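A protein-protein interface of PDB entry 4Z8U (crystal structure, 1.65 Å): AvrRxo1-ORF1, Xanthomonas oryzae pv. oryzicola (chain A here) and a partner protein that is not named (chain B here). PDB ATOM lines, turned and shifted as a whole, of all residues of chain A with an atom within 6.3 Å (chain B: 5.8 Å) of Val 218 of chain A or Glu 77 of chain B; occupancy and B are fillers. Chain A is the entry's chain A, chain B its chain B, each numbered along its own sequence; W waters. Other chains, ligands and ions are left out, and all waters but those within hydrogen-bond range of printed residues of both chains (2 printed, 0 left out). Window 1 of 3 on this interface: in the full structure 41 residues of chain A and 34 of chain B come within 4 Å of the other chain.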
ATOM      1  N   ASN A  73     -17.152  18.756   9.617  1.00  0.00           N
ATOM      2  CA  ASN A  73     -17.725  19.984   9.035  1.00  0.00           C
ATOM      3  C   ASN A  73     -17.043  20.528   7.769  1.00  0.00           C
ATOM      4  O   ASN A  73     -15.943  20.128   7.381  1.00  0.00           O
ATOM      5  CB  ASN A  73     -17.766  21.041  10.168  1.00  0.00           C
ATOM      6  CG  ASN A  73     -18.800  22.131   9.859  1.00  0.00           C
ATOM      7  OD1 ASN A  73     -19.763  21.937   9.170  1.00  0.00           O
ATOM      8  ND2 ASN A  73     -18.539  23.340  10.438  1.00  0.00           N
ATOM      9  N   ARG A 162     -25.100  13.701  12.123  1.00  0.00           N
ATOM     10  CA  ARG A 162     -26.148  13.212  13.071  1.00  0.00           C
ATOM     11  C   ARG A 162     -26.274  11.728  13.265  1.00  0.00           C
ATOM     12  O   ARG A 162     -25.854  10.948  12.406  1.00  0.00           O
ATOM     13  CB  ARG A 162     -27.498  13.785  12.705  1.00  0.00           C
ATOM     14  CG  ARG A 162     -27.450  15.309  12.630  1.00  0.00           C
ATOM     15  CD  ARG A 162     -28.762  15.980  12.907  1.00  0.00           C
ATOM     16  NE  ARG A 162     -28.713  17.390  12.575  1.00  0.00           N
ATOM     17  CZ  ARG A 162     -28.446  18.336  13.448  1.00  0.00           C
ATOM     18  NH1 ARG A 162     -28.430  19.582  13.033  1.00  0.00           N
ATOM     19  NH2 ARG A 162     -28.207  18.053  14.716  1.00  0.00           N
ATOM     20  N   PRO A 211     -25.116  30.036   8.293  1.00  0.00           N
ATOM     21  CA  PRO A 211     -25.836  29.066   9.082  1.00  0.00           C
ATOM     22  C   PRO A 211     -25.448  27.598   8.780  1.00  0.00           C
ATOM     23  O   PRO A 211     -25.527  26.779   9.735  1.00  0.00           O
ATOM     24  CB  PRO A 211     -27.303  29.309   8.733  1.00  0.00           C
ATOM     25  CG  PRO A 211     -27.376  30.749   8.282  1.00  0.00           C
ATOM     26  CD  PRO A 211     -26.045  30.914   7.547  1.00  0.00           C
ATOM     27  N   VAL A 213     -22.512  26.420   8.009  1.00  0.00           N
ATOM     28  CA  VAL A 213     -21.231  26.106   8.662  1.00  0.00           C
ATOM     29  C   VAL A 213     -21.325  26.054  10.177  1.00  0.00           C
ATOM     30  O   VAL A 213     -20.775  25.171  10.827  1.00  0.00           O
ATOM     31  CB  VAL A 213     -20.143  27.152   8.211  1.00  0.00           C
ATOM     32  CG1 VAL A 213     -18.741  26.727   8.760  1.00  0.00           C
ATOM     33  CG2 VAL A 213     -20.152  27.240   6.713  1.00  0.00           C
ATOM     34  N   SER A 214     -22.138  26.966  10.791  1.00  0.00           N
ATOM     35  CA  SER A 214     -22.263  26.990  12.244  1.00  0.00           C
ATOM     36  C   SER A 214     -23.139  25.857  12.670  1.00  0.00           C
ATOM     37  O   SER A 214     -22.807  25.132  13.664  1.00  0.00           O
ATOM     38  CB  SER A 214     -22.892  28.339  12.641  1.00  0.00           C
ATOM     39  OG  SER A 214     -22.877  28.454  14.033  1.00  0.00           O
ATOM     40  N   SER A 215     -24.251  25.670  11.999  1.00  0.00           N
ATOM     41  CA  SER A 215     -25.125  24.541  12.456  1.00  0.00           C
ATOM     42  C   SER A 215     -24.411  23.183  12.197  1.00  0.00           C
ATOM     43  O   SER A 215     -24.571  22.258  12.988  1.00  0.00           O
ATOM     44  CB  SER A 215     -26.518  24.522  11.822  1.00  0.00           C
ATOM     45  OG  SER A 215     -27.299  25.544  12.505  1.00  0.00           O
ATOM     46  N   GLY A 216     -23.608  23.112  11.121  1.00  0.00           N
ATOM     47  CA  GLY A 216     -22.762  21.907  10.847  1.00  0.00           C
ATOM     48  C   GLY A 216     -21.790  21.649  11.964  1.00  0.00           C
ATOM     49  O   GLY A 216     -21.567  20.495  12.386  1.00  0.00           O
ATOM     50  N   PHE A 217     -21.174  22.717  12.451  1.00  0.00           N
ATOM     51  CA  PHE A 217     -20.184  22.645  13.561  1.00  0.00           C
ATOM     52  C   PHE A 217     -20.839  22.109  14.814  1.00  0.00           C
ATOM     53  O   PHE A 217     -20.283  21.258  15.451  1.00  0.00           O
ATOM     54  CB  PHE A 217     -19.649  24.045  13.755  1.00  0.00           C
ATOM     55  CG  PHE A 217     -18.767  24.186  14.980  1.00  0.00           C
ATOM     56  CD1 PHE A 217     -17.408  23.935  14.888  1.00  0.00           C
ATOM     57  CD2 PHE A 217     -19.295  24.740  16.142  1.00  0.00           C
ATOM     58  CE1 PHE A 217     -16.561  24.118  16.017  1.00  0.00           C
ATOM     59  CE2 PHE A 217     -18.447  24.945  17.251  1.00  0.00           C
ATOM     60  CZ  PHE A 217     -17.060  24.668  17.161  1.00  0.00           C
ATOM     61  N   VAL A 218     -21.968  22.728  15.166  1.00  0.00           N
ATOM     62  CA  VAL A 218     -22.662  22.305  16.338  1.00  0.00           C
ATOM     63  C   VAL A 218     -23.044  20.848  16.245  1.00  0.00           C
ATOM     64  O   VAL A 218     -22.856  20.087  17.228  1.00  0.00           O
ATOM     65  CB  VAL A 218     -23.912  23.210  16.610  1.00  0.00           C
ATOM     66  CG1 VAL A 218     -24.740  22.595  17.774  1.00  0.00           C
ATOM     67  CG2 VAL A 218     -23.423  24.675  16.921  1.00  0.00           C
ATOM     68  N   ALA A 219     -23.547  20.422  15.092  1.00  0.00           N
ATOM     69  CA  ALA A 219     -24.083  19.028  14.968  1.00  0.00           C
ATOM     70  C   ALA A 219     -22.913  18.040  15.002  1.00  0.00           C
ATOM     71  O   ALA A 219     -22.972  16.995  15.721  1.00  0.00           O
ATOM     72  CB  ALA A 219     -24.854  18.899  13.705  1.00  0.00           C
ATOM     73  N   VAL A 220     -21.813  18.405  14.348  1.00  0.00           N
ATOM     74  CA  VAL A 220     -20.692  17.443  14.261  1.00  0.00           C
ATOM     75  C   VAL A 220     -20.042  17.271  15.603  1.00  0.00           C
ATOM     76  O   VAL A 220     -19.661  16.174  15.985  1.00  0.00           O
ATOM     77  CB  VAL A 220     -19.707  17.882  13.125  1.00  0.00           C
ATOM     78  CG1 VAL A 220     -18.752  18.934  13.580  1.00  0.00           C
ATOM     79  CG2 VAL A 220     -18.929  16.651  12.616  1.00  0.00           C
ATOM     80  N   ARG A 221     -19.897  18.368  16.385  1.00  0.00           N
ATOM     81  CA  ARG A 221     -19.279  18.256  17.683  1.00  0.00           C
ATOM     82  C   ARG A 221     -20.246  17.518  18.692  1.00  0.00           C
ATOM     83  O   ARG A 221     -19.787  16.647  19.436  1.00  0.00           O
ATOM     84  CB  ARG A 221     -18.901  19.642  18.262  1.00  0.00           C
ATOM     85  CG  ARG A 221     -17.670  20.106  17.503  1.00  0.00           C
ATOM     86  CD  ARG A 221     -16.847  20.898  18.387  1.00  0.00           C
ATOM     87  NE  ARG A 221     -15.566  21.287  17.780  1.00  0.00           N
ATOM     88  CZ  ARG A 221     -14.848  22.238  18.274  1.00  0.00           C
ATOM     89  NH1 ARG A 221     -15.211  22.865  19.386  1.00  0.00           N
ATOM     90  NH2 ARG A 221     -13.730  22.607  17.611  1.00  0.00           N
ATOM     91  N   SER A 222     -21.532  17.874  18.662  1.00  0.00           N
ATOM     92  CA  SER A 222     -22.451  17.333  19.701  1.00  0.00           C
ATOM     93  C   SER A 222     -22.650  15.848  19.565  1.00  0.00           C
ATOM     94  O   SER A 222     -22.972  15.181  20.578  1.00  0.00           O
ATOM     95  CB  SER A 222     -23.850  18.023  19.671  1.00  0.00           C
ATOM     96  OG  SER A 222     -23.611  19.453  19.926  1.00  0.00           O
ATOM     97  N   ASN A 223     -22.563  15.336  18.334  1.00  0.00           N
ATOM     98  CA  ASN A 223     -22.822  13.927  18.089  1.00  0.00           C
ATOM     99  C   ASN A 223     -21.537  13.084  17.991  1.00  0.00           C
ATOM    100  O   ASN A 223     -21.569  11.909  17.657  1.00  0.00           O
ATOM    101  CB  ASN A 223     -23.679  13.780  16.843  1.00  0.00           C
ATOM    102  CG  ASN A 223     -25.057  14.290  17.103  1.00  0.00           C
ATOM    103  OD1 ASN A 223     -25.789  13.695  17.921  1.00  0.00           O
ATOM    104  ND2 ASN A 223     -25.416  15.364  16.528  1.00  0.00           N
ATOM    105  N   PRO A 276     -19.770  21.977  21.492  1.00  0.00           N
ATOM    106  CA  PRO A 276     -19.960  23.159  20.599  1.00  0.00           C
ATOM    107  C   PRO A 276     -19.643  24.585  21.192  1.00  0.00           C
ATOM    108  O   PRO A 276     -19.639  25.584  20.456  1.00  0.00           O
ATOM    109  CB  PRO A 276     -21.412  23.027  20.226  1.00  0.00           C
ATOM    110  CG  PRO A 276     -22.042  22.372  21.427  1.00  0.00           C
ATOM    111  CD  PRO A 276     -21.050  21.316  21.836  1.00  0.00           C
ATOM    112  N   LEU A 278     -21.120  26.600  23.188  1.00  0.00           N
ATOM    113  CA  LEU A 278     -22.208  27.573  22.996  1.00  0.00           C
ATOM    114  C   LEU A 278     -22.457  28.417  24.276  1.00  0.00           C
ATOM    115  O   LEU A 278     -22.048  28.027  25.372  1.00  0.00           O
ATOM    116  CB  LEU A 278     -23.521  26.819  22.705  1.00  0.00           C
ATOM    117  CG  LEU A 278     -23.363  25.919  21.521  1.00  0.00           C
ATOM    118  CD1 LEU A 278     -24.652  25.140  21.325  1.00  0.00           C
ATOM    119  CD2 LEU A 278     -23.119  26.815  20.309  1.00  0.00           C
ATOM    120  N   GLY A 282     -24.369  34.043  22.440  1.00  0.00           N
ATOM    121  CA  GLY A 282     -23.054  34.351  21.769  1.00  0.00           C
ATOM    122  C   GLY A 282     -23.293  34.493  20.273  1.00  0.00           C
ATOM    123  O   GLY A 282     -24.134  33.743  19.738  1.00  0.00           O
ATOM    124  N   ARG B  72     -34.341  22.100  19.612  1.00  0.00           N
ATOM    125  CA  ARG B  72     -33.066  22.448  20.179  1.00  0.00           C
ATOM    126  C   ARG B  72     -32.326  23.482  19.326  1.00  0.00           C
ATOM    127  O   ARG B  72     -31.848  24.417  19.830  1.00  0.00           O
ATOM    128  CB  ARG B  72     -32.222  21.206  20.369  1.00  0.00           C
ATOM    129  CG  ARG B  72     -30.974  21.439  21.047  1.00  0.00           C
ATOM    130  CD  ARG B  72     -30.229  20.199  21.291  1.00  0.00           C
ATOM    131  NE  ARG B  72     -30.648  19.690  22.553  1.00  0.00           N
ATOM    132  CZ  ARG B  72     -30.180  20.123  23.710  1.00  0.00           C
ATOM    133  NH1 ARG B  72     -30.677  19.597  24.770  1.00  0.00           N
ATOM    134  NH2 ARG B  72     -29.207  21.031  23.795  1.00  0.00           N
ATOM    135  N   MET B  73     -32.257  23.280  18.032  1.00  0.00           N
ATOM    136  CA  MET B  73     -31.628  24.262  17.109  1.00  0.00           C
ATOM    137  C   MET B  73     -32.318  25.610  17.302  1.00  0.00           C
ATOM    138  O   MET B  73     -31.694  26.665  17.361  1.00  0.00           O
ATOM    139  CB  MET B  73     -31.681  23.736  15.649  1.00  0.00           C
ATOM    140  CG  MET B  73     -31.054  24.772  14.760  1.00  0.00           C
ATOM    141  SD  MET B  73     -31.353  24.067  12.913  1.00  0.00           S
ATOM    142  CE  MET B  73     -30.245  22.516  13.127  1.00  0.00           C
ATOM    143  N   TYR B  74     -33.676  25.596  17.331  1.00  0.00           N
ATOM    144  CA  TYR B  74     -34.437  26.841  17.412  1.00  0.00           C
ATOM    145  C   TYR B  74     -34.069  27.647  18.669  1.00  0.00           C
ATOM    146  O   TYR B  74     -33.792  28.834  18.607  1.00  0.00           O
ATOM    147  CB  TYR B  74     -35.941  26.435  17.468  1.00  0.00           C
ATOM    148  CG  TYR B  74     -36.947  27.629  17.577  1.00  0.00           C
ATOM    149  CD1 TYR B  74     -37.034  28.576  16.586  1.00  0.00           C
ATOM    150  CD2 TYR B  74     -37.754  27.739  18.686  1.00  0.00           C
ATOM    151  CE1 TYR B  74     -37.966  29.626  16.633  1.00  0.00           C
ATOM    152  CE2 TYR B  74     -38.733  28.769  18.769  1.00  0.00           C
ATOM    153  CZ  TYR B  74     -38.799  29.714  17.760  1.00  0.00           C
ATOM    154  OH  TYR B  74     -39.700  30.762  17.794  1.00  0.00           O
ATOM    155  N   TYR B  75     -34.046  26.969  19.791  1.00  0.00           N
ATOM    156  CA  TYR B  75     -33.779  27.671  21.040  1.00  0.00           C
ATOM    157  C   TYR B  75     -32.285  27.954  21.315  1.00  0.00           C
ATOM    158  O   TYR B  75     -31.970  29.038  21.739  1.00  0.00           O
ATOM    159  CB  TYR B  75     -34.309  26.854  22.205  1.00  0.00           C
ATOM    160  CG  TYR B  75     -35.845  27.031  22.291  1.00  0.00           C
ATOM    161  CD1 TYR B  75     -36.418  28.325  22.417  1.00  0.00           C
ATOM    162  CD2 TYR B  75     -36.663  25.940  22.190  1.00  0.00           C
ATOM    163  CE1 TYR B  75     -37.816  28.483  22.465  1.00  0.00           C
ATOM    164  CE2 TYR B  75     -38.067  26.091  22.222  1.00  0.00           C
ATOM    165  CZ  TYR B  75     -38.605  27.357  22.413  1.00  0.00           C
ATOM    166  OH  TYR B  75     -39.965  27.567  22.405  1.00  0.00           O
ATOM    167  N   VAL B  76     -31.454  26.937  21.094  1.00  0.00           N
ATOM    168  CA  VAL B  76     -30.017  27.003  21.477  1.00  0.00           C
ATOM    169  C   VAL B  76     -29.185  27.707  20.430  1.00  0.00           C
ATOM    170  O   VAL B  76     -28.364  28.571  20.775  1.00  0.00           O
ATOM    171  CB  VAL B  76     -29.437  25.625  21.860  1.00  0.00           C
ATOM    172  CG1 VAL B  76     -27.969  25.657  22.212  1.00  0.00           C
ATOM    173  CG2 VAL B  76     -30.236  24.966  22.989  1.00  0.00           C
ATOM    174  N   GLU B  77     -29.360  27.332  19.172  1.00  0.00           N
ATOM    175  CA  GLU B  77     -28.508  27.928  18.128  1.00  0.00           C
ATOM    176  C   GLU B  77     -28.977  29.240  17.631  1.00  0.00           C
ATOM    177  O   GLU B  77     -28.165  30.005  17.072  1.00  0.00           O
ATOM    178  CB  GLU B  77     -28.353  26.939  16.952  1.00  0.00           C
ATOM    179  CG  GLU B  77     -27.572  25.719  17.333  1.00  0.00           C
ATOM    180  CD  GLU B  77     -27.415  24.802  16.115  1.00  0.00           C
ATOM    181  OE1 GLU B  77     -27.798  23.584  16.179  1.00  0.00           O
ATOM    182  OE2 GLU B  77     -26.865  25.333  15.073  1.00  0.00           O
ATOM    183  N   TYR B  78     -30.283  29.555  17.776  1.00  0.00           N
ATOM    184  CA  TYR B  78     -30.782  30.750  17.090  1.00  0.00           C
ATOM    185  C   TYR B  78     -31.563  31.625  18.060  1.00  0.00           C
ATOM    186  O   TYR B  78     -32.780  31.848  17.876  1.00  0.00           O
ATOM    187  CB  TYR B  78     -31.626  30.393  15.837  1.00  0.00           C
ATOM    188  CG  TYR B  78     -30.733  29.787  14.732  1.00  0.00           C
ATOM    189  CD1 TYR B  78     -30.008  30.637  13.821  1.00  0.00           C
ATOM    190  CD2 TYR B  78     -30.528  28.405  14.658  1.00  0.00           C
ATOM    191  CE1 TYR B  78     -29.105  30.104  12.928  1.00  0.00           C
ATOM    192  CE2 TYR B  78     -29.686  27.842  13.714  1.00  0.00           C
ATOM    193  CZ  TYR B  78     -28.960  28.725  12.850  1.00  0.00           C
ATOM    194  OH  TYR B  78     -28.079  28.234  11.916  1.00  0.00           O
ATOM    195  N   PRO B  79     -30.896  32.002  19.182  1.00  0.00           N
ATOM    196  CA  PRO B  79     -31.645  32.683  20.266  1.00  0.00           C
ATOM    197  C   PRO B  79     -32.280  34.019  19.837  1.00  0.00           C
ATOM    198  O   PRO B  79     -33.257  34.429  20.485  1.00  0.00           O
ATOM    199  CB  PRO B  79     -30.567  32.939  21.326  1.00  0.00           C
ATOM    200  CG  PRO B  79     -29.280  32.980  20.543  1.00  0.00           C
ATOM    201  CD  PRO B  79     -29.435  31.960  19.444  1.00  0.00           C
HETATM  202  O   HOH W   1     -25.350  27.581  14.888  1.00  0.00           O
HETATM  203  O   HOH W   2     -27.011  21.911  14.419  1.00  0.00           O
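Glu 77 of chain B touches just these residues of chain A: Ser 215 (2.6 Å) and Val 218 (3.6 Å). Printed residues of chain B within 4 Å of Leu 278 of chain A: Val 76 (3.5 Å). Printed residues of chain B within 4 Å of Ser 215 of chain A: Glu 77 (2.6 Å) and Tyr 78 (2.9 Å). Of the printed residues of chain A, Tyr 78 of chain B touches Pro 211 and Ser 215. The nearest residue of chain A that does not touch Glu 77 of chain B is Ser 214 of chain A (4.3 Å). The nearest printed residue of chain A that does not touch Tyr 78 of chain B is Ser 214 of chain A (5.2 Å).
The side-chain hydroxyl of Ser 222 of chain A sits at hydrogen-bond distance from the backbone carbonyl oxygen of Val 218 of chain A (2.9 Å). O of Met 73 of chain B lies within hydrogen-bond range of N of Tyr 78 of chain B, 3.2 Å away.
OG of Ser 215 of chain A is in hydrogen-bond range of OE2 of Glu 77 of chain B. OH of Tyr 78 of chain B is in hydrogen-bond range of OG of Ser 215 of chain A, 2.9 Å away.
Printed residues of chain A that touch a printed residue of chain B: Arg 162, Pro 211, Ser 215, Val 218 and Leu 278. Hydrophobic or aromatic side chains of chain A within 4 Å of the printed part of chain B: Pro 211, Val 218 and Leu 278. Among the printed residues, 6 pairs touch across the chains.
Among the printed residues, pairs that only touch across the chains: Pro 211 of chain A with Tyr 78 of chain B, Arg 162 of chain A with Met 73 of chain B, Leu 278 of chain A with Val 76 of chain B and Val 218 of chain A with Glu 77 of chain B.
Water W2 lies within hydrogen-bond range of OE1 of Glu 77 of chain B, O of Ser 215 of chain A and NH1 of Arg 162 of chain A. Water W1 lies within hydrogen-bond range of OE2 of Glu 77 of chain B (2.7 Å) and OG of Ser 214 of chain A (2.8 Å).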
